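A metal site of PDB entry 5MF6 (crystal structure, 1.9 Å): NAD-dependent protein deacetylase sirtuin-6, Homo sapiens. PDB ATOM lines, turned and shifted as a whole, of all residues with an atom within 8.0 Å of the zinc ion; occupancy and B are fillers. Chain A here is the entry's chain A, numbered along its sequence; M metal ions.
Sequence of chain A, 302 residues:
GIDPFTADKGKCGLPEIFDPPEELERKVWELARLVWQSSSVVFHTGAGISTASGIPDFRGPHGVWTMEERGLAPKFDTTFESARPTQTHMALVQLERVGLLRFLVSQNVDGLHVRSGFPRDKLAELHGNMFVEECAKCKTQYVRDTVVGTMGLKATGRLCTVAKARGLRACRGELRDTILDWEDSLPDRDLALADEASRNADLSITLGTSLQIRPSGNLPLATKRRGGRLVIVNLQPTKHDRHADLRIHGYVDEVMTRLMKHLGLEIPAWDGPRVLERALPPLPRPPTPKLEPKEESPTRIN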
ATOM      1  N   GLU A 134     -13.587  -1.345  14.681  1.00  0.00           N
ATOM      2  CA  GLU A 134     -14.426  -0.277  15.099  1.00  0.00           C
ATOM      3  C   GLU A 134     -13.654   0.553  16.152  1.00  0.00           C
ATOM      4  O   GLU A 134     -13.081  -0.059  17.071  1.00  0.00           O
ATOM      5  CB  GLU A 134     -15.735  -0.778  15.695  1.00  0.00           C
ATOM      6  CG  GLU A 134     -16.594   0.332  16.317  1.00  0.00           C
ATOM      7  CD  GLU A 134     -18.095   0.006  16.508  1.00  0.00           C
ATOM      8  OE1 GLU A 134     -18.731  -0.704  15.697  1.00  0.00           O
ATOM      9  OE2 GLU A 134     -18.660   0.579  17.457  1.00  0.00           O
ATOM     10  N   CYS A 135     -13.679   1.871  15.979  1.00  0.00           N
ATOM     11  CA  CYS A 135     -13.007   2.838  16.886  1.00  0.00           C
ATOM     12  C   CYS A 135     -13.844   2.977  18.151  1.00  0.00           C
ATOM     13  O   CYS A 135     -15.021   3.329  18.114  1.00  0.00           O
ATOM     14  CB  CYS A 135     -12.844   4.227  16.248  1.00  0.00           C
ATOM     15  SG  CYS A 135     -12.146   5.496  17.339  1.00  0.00           S
ATOM     16  N   ALA A 136     -13.238   2.608  19.268  1.00  0.00           N
ATOM     17  CA  ALA A 136     -13.866   2.733  20.601  1.00  0.00           C
ATOM     18  C   ALA A 136     -14.275   4.185  20.938  1.00  0.00           C
ATOM     19  O   ALA A 136     -15.188   4.382  21.755  1.00  0.00           O
ATOM     20  CB  ALA A 136     -12.922   2.178  21.636  1.00  0.00           C
ATOM     21  N   LYS A 137     -13.662   5.183  20.285  1.00  0.00           N
ATOM     22  CA  LYS A 137     -13.889   6.579  20.637  1.00  0.00           C
ATOM     23  C   LYS A 137     -14.933   7.182  19.782  1.00  0.00           C
ATOM     24  O   LYS A 137     -15.879   7.698  20.322  1.00  0.00           O
ATOM     25  CB  LYS A 137     -12.570   7.399  20.606  1.00  0.00           C
ATOM     26  CG  LYS A 137     -11.574   6.836  21.635  1.00  0.00           C
ATOM     27  CD  LYS A 137     -10.592   7.843  22.229  1.00  0.00           C
ATOM     28  CE  LYS A 137     -10.104   7.388  23.611  1.00  0.00           C
ATOM     29  NZ  LYS A 137      -8.627   7.499  23.773  1.00  0.00           N
ATOM     30  N   CYS A 138     -14.791   7.127  18.459  1.00  0.00           N
ATOM     31  CA  CYS A 138     -15.785   7.748  17.572  1.00  0.00           C
ATOM     32  C   CYS A 138     -16.741   6.734  16.925  1.00  0.00           C
ATOM     33  O   CYS A 138     -17.681   7.140  16.336  1.00  0.00           O
ATOM     34  CB  CYS A 138     -15.138   8.623  16.529  1.00  0.00           C
ATOM     35  SG  CYS A 138     -14.225   7.802  15.185  1.00  0.00           S
ATOM     36  N   LYS A 139     -16.532   5.422  17.087  1.00  0.00           N
ATOM     37  CA  LYS A 139     -17.430   4.387  16.526  1.00  0.00           C
ATOM     38  C   LYS A 139     -17.308   4.135  15.029  1.00  0.00           C
ATOM     39  O   LYS A 139     -18.035   3.260  14.484  1.00  0.00           O
ATOM     40  CB  LYS A 139     -18.917   4.617  16.925  1.00  0.00           C
ATOM     41  CG  LYS A 139     -19.157   4.851  18.411  1.00  0.00           C
ATOM     42  CD  LYS A 139     -18.749   3.613  19.230  1.00  0.00           C
ATOM     43  CE  LYS A 139     -18.259   3.932  20.636  1.00  0.00           C
ATOM     44  NZ  LYS A 139     -19.311   3.695  21.655  1.00  0.00           N
ATOM     45  N   THR A 140     -16.362   4.809  14.361  1.00  0.00           N
ATOM     46  CA  THR A 140     -16.133   4.660  12.939  1.00  0.00           C
ATOM     47  C   THR A 140     -15.598   3.251  12.640  1.00  0.00           C
ATOM     48  O   THR A 140     -14.702   2.791  13.314  1.00  0.00           O
ATOM     49  CB  THR A 140     -15.077   5.699  12.402  1.00  0.00           C
ATOM     50  OG1 THR A 140     -15.594   7.032  12.527  1.00  0.00           O
ATOM     51  CG2 THR A 140     -14.791   5.513  10.930  1.00  0.00           C
ATOM     52  N   GLN A 141     -16.125   2.626  11.575  1.00  0.00           N
ATOM     53  CA  GLN A 141     -15.820   1.241  11.186  1.00  0.00           C
ATOM     54  C   GLN A 141     -14.843   1.212  10.039  1.00  0.00           C
ATOM     55  O   GLN A 141     -14.801   2.113   9.230  1.00  0.00           O
ATOM     56  CB  GLN A 141     -17.145   0.412  10.936  1.00  0.00           C
ATOM     57  CG  GLN A 141     -17.971   0.280  12.192  1.00  0.00           C
ATOM     58  CD  GLN A 141     -19.193  -0.607  12.030  1.00  0.00           C
ATOM     59  OE1 GLN A 141     -19.710  -0.715  10.951  1.00  0.00           O
ATOM     60  NE2 GLN A 141     -19.584  -1.303  13.093  1.00  0.00           N
ATOM     61  N   TYR A 142     -13.893   0.311  10.091  1.00  0.00           N
ATOM     62  CA  TYR A 142     -13.016   0.055   8.991  1.00  0.00           C
ATOM     63  C   TYR A 142     -13.293  -1.355   8.491  1.00  0.00           C
ATOM     64  O   TYR A 142     -13.215  -2.370   9.287  1.00  0.00           O
ATOM     65  CB  TYR A 142     -11.565   0.247   9.439  1.00  0.00           C
ATOM     66  CG  TYR A 142     -11.290   1.622   9.987  1.00  0.00           C
ATOM     67  CD1 TYR A 142     -11.782   2.027  11.199  1.00  0.00           C
ATOM     68  CD2 TYR A 142     -10.480   2.545   9.240  1.00  0.00           C
ATOM     69  CE1 TYR A 142     -11.524   3.325  11.689  1.00  0.00           C
ATOM     70  CE2 TYR A 142     -10.218   3.811   9.702  1.00  0.00           C
ATOM     71  CZ  TYR A 142     -10.743   4.218  10.908  1.00  0.00           C
ATOM     72  OH  TYR A 142     -10.430   5.490  11.319  1.00  0.00           O
ATOM     73  N   LEU A 159      -4.886   2.237  15.220  1.00  0.00           N
ATOM     74  CA  LEU A 159      -5.575   3.447  15.627  1.00  0.00           C
ATOM     75  C   LEU A 159      -6.377   4.081  14.531  1.00  0.00           C
ATOM     76  O   LEU A 159      -6.059   3.976  13.333  1.00  0.00           O
ATOM     77  CB  LEU A 159      -4.578   4.518  16.125  1.00  0.00           C
ATOM     78  CG  LEU A 159      -3.646   4.099  17.249  1.00  0.00           C
ATOM     79  CD1 LEU A 159      -2.766   5.295  17.587  1.00  0.00           C
ATOM     80  CD2 LEU A 159      -4.449   3.651  18.472  1.00  0.00           C
ATOM     81  N   CYS A 160      -7.307   4.895  14.980  1.00  0.00           N
ATOM     82  CA  CYS A 160      -8.244   5.563  14.160  1.00  0.00           C
ATOM     83  C   CYS A 160      -7.561   6.718  13.403  1.00  0.00           C
ATOM     84  O   CYS A 160      -6.760   7.425  13.973  1.00  0.00           O
ATOM     85  CB  CYS A 160      -9.300   6.094  15.056  1.00  0.00           C
ATOM     86  SG  CYS A 160     -10.707   6.686  14.167  1.00  0.00           S
ATOM     87  N   THR A 161      -7.898   6.890  12.141  1.00  0.00           N
ATOM     88  CA  THR A 161      -7.367   7.931  11.352  1.00  0.00           C
ATOM     89  C   THR A 161      -8.405   8.932  10.910  1.00  0.00           C
ATOM     90  O   THR A 161      -8.162   9.684   9.973  1.00  0.00           O
ATOM     91  CB  THR A 161      -6.633   7.323  10.134  1.00  0.00           C
ATOM     92  OG1 THR A 161      -7.578   6.576   9.362  1.00  0.00           O
ATOM     93  CG2 THR A 161      -5.455   6.432  10.590  1.00  0.00           C
ATOM     94  N   VAL A 162      -9.554   9.010  11.587  1.00  0.00           N
ATOM     95  CA  VAL A 162     -10.561  10.025  11.241  1.00  0.00           C
ATOM     96  C   VAL A 162      -9.972  11.443  11.505  1.00  0.00           C
ATOM     97  O   VAL A 162      -9.219  11.600  12.473  1.00  0.00           O
ATOM     98  CB  VAL A 162     -11.904   9.825  11.984  1.00  0.00           C
ATOM     99  CG1 VAL A 162     -12.882  10.973  11.757  1.00  0.00           C
ATOM    100  CG2 VAL A 162     -12.549   8.559  11.467  1.00  0.00           C
ATOM    101  N   ALA A 163     -10.343  12.392  10.605  1.00  0.00           N
ATOM    102  CA  ALA A 163      -9.822  13.785  10.548  1.00  0.00           C
ATOM    103  C   ALA A 163     -10.091  14.618  11.798  1.00  0.00           C
ATOM    104  O   ALA A 163     -11.253  14.876  12.116  1.00  0.00           O
ATOM    105  CB  ALA A 163     -10.390  14.520   9.321  1.00  0.00           C
ATOM    106  N   CYS A 171      -8.311  11.544  15.352  1.00  0.00           N
ATOM    107  CA  CYS A 171      -8.936  10.810  16.457  1.00  0.00           C
ATOM    108  C   CYS A 171      -7.970   9.940  17.289  1.00  0.00           C
ATOM    109  O   CYS A 171      -7.914  10.034  18.518  1.00  0.00           O
ATOM    110  CB  CYS A 171     -10.087   9.986  15.902  1.00  0.00           C
ATOM    111  SG  CYS A 171     -10.945   8.987  17.127  1.00  0.00           S
ATOM    112  N   ARG A 172      -7.192   9.086  16.632  1.00  0.00           N
ATOM    113  CA  ARG A 172      -6.302   8.117  17.315  1.00  0.00           C
ATOM    114  C   ARG A 172      -6.951   7.220  18.407  1.00  0.00           C
ATOM    115  O   ARG A 172      -6.252   6.663  19.232  1.00  0.00           O
ATOM    116  CB  ARG A 172      -5.005   8.804  17.818  1.00  0.00           C
ATOM    117  CG  ARG A 172      -4.519   9.898  16.861  1.00  0.00           C
ATOM    118  CD  ARG A 172      -3.093  10.428  17.094  1.00  0.00           C
ATOM    119  NE  ARG A 172      -2.071   9.464  16.631  1.00  0.00           N
ATOM    120  CZ  ARG A 172      -1.381   8.608  17.400  1.00  0.00           C
ATOM    121  NH1 ARG A 172      -1.562   8.528  18.721  1.00  0.00           N
ATOM    122  NH2 ARG A 172      -0.506   7.796  16.839  1.00  0.00           N
ATOM    123  N   GLY A 173      -8.260   6.994  18.337  1.00  0.00           N
ATOM    124  CA  GLY A 173      -8.939   5.985  19.215  1.00  0.00           C
ATOM    125  C   GLY A 173      -8.434   4.546  18.986  1.00  0.00           C
ATOM    126  O   GLY A 173      -7.848   4.282  17.925  1.00  0.00           O
ATOM    127  N   GLU A 174      -8.587   3.646  19.997  1.00  0.00           N
ATOM    128  CA  GLU A 174      -8.207   2.222  19.873  1.00  0.00           C
ATOM    129  C   GLU A 174      -9.210   1.564  18.891  1.00  0.00           C
ATOM    130  O   GLU A 174     -10.433   1.810  19.001  1.00  0.00           O
ATOM    131  CB  GLU A 174      -8.189   1.453  21.199  1.00  0.00           C
ATOM    132  N   LEU A 175      -8.686   0.872  17.877  1.00  0.00           N
ATOM    133  CA  LEU A 175      -9.533   0.010  17.004  1.00  0.00           C
ATOM    134  C   LEU A 175      -9.728  -1.340  17.676  1.00  0.00           C
ATOM    135  O   LEU A 175      -8.778  -1.956  18.183  1.00  0.00           O
ATOM    136  CB  LEU A 175      -8.930  -0.150  15.613  1.00  0.00           C
ATOM    137  CG  LEU A 175      -8.778   1.143  14.804  1.00  0.00           C
ATOM    138  CD1 LEU A 175      -8.540   0.790  13.354  1.00  0.00           C
ATOM    139  CD2 LEU A 175      -9.981   2.067  14.965  1.00  0.00           C
HETATM  140 ZN    ZN M   1     -12.065   7.302  15.896  1.00  0.00          ZN
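The zinc ion is bound by the side-chain sulfur of Cys 160 (2.3 Å), the side-chain sulfur of Cys 135 (2.3 Å), the side-chain sulfur of Cys 138 (2.3 Å) and the side-chain sulfur of Cys 171 (2.4 Å).
The backbone carbonyl oxygen of Gly 173 sits at hydrogen-bond distance from the backbone NH of Cys 160 (3.1 Å). The side-chain sulfur of Cys 160 sits close to the backbone NH of Val 162, at 3.7 Å. OH of Tyr 142 sits close to SG of Cys 160, 3.1 Å away. N of Arg 172 sits at hydrogen-bond distance from O of Cys 160 (3.2 Å). The side-chain sulfur of Cys 135 sits close to the backbone NH of Lys 137. The backbone carbonyl oxygen (O) of Thr 140 lies within hydrogen-bond range of the backbone NH (N) of Cys 135. The side-chain sulfur (SG) of Cys 171 sits close to the backbone NH (N) of Gly 173, 3.6 Å away. The backbone NH (N) of Cys 171 lies within hydrogen-bond range of the backbone carbonyl oxygen (O) of Val 162 (3.0 Å).
Within 4 Å of the zinc ion: Cys 135, Cys 138, Cys 160 and Cys 171.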
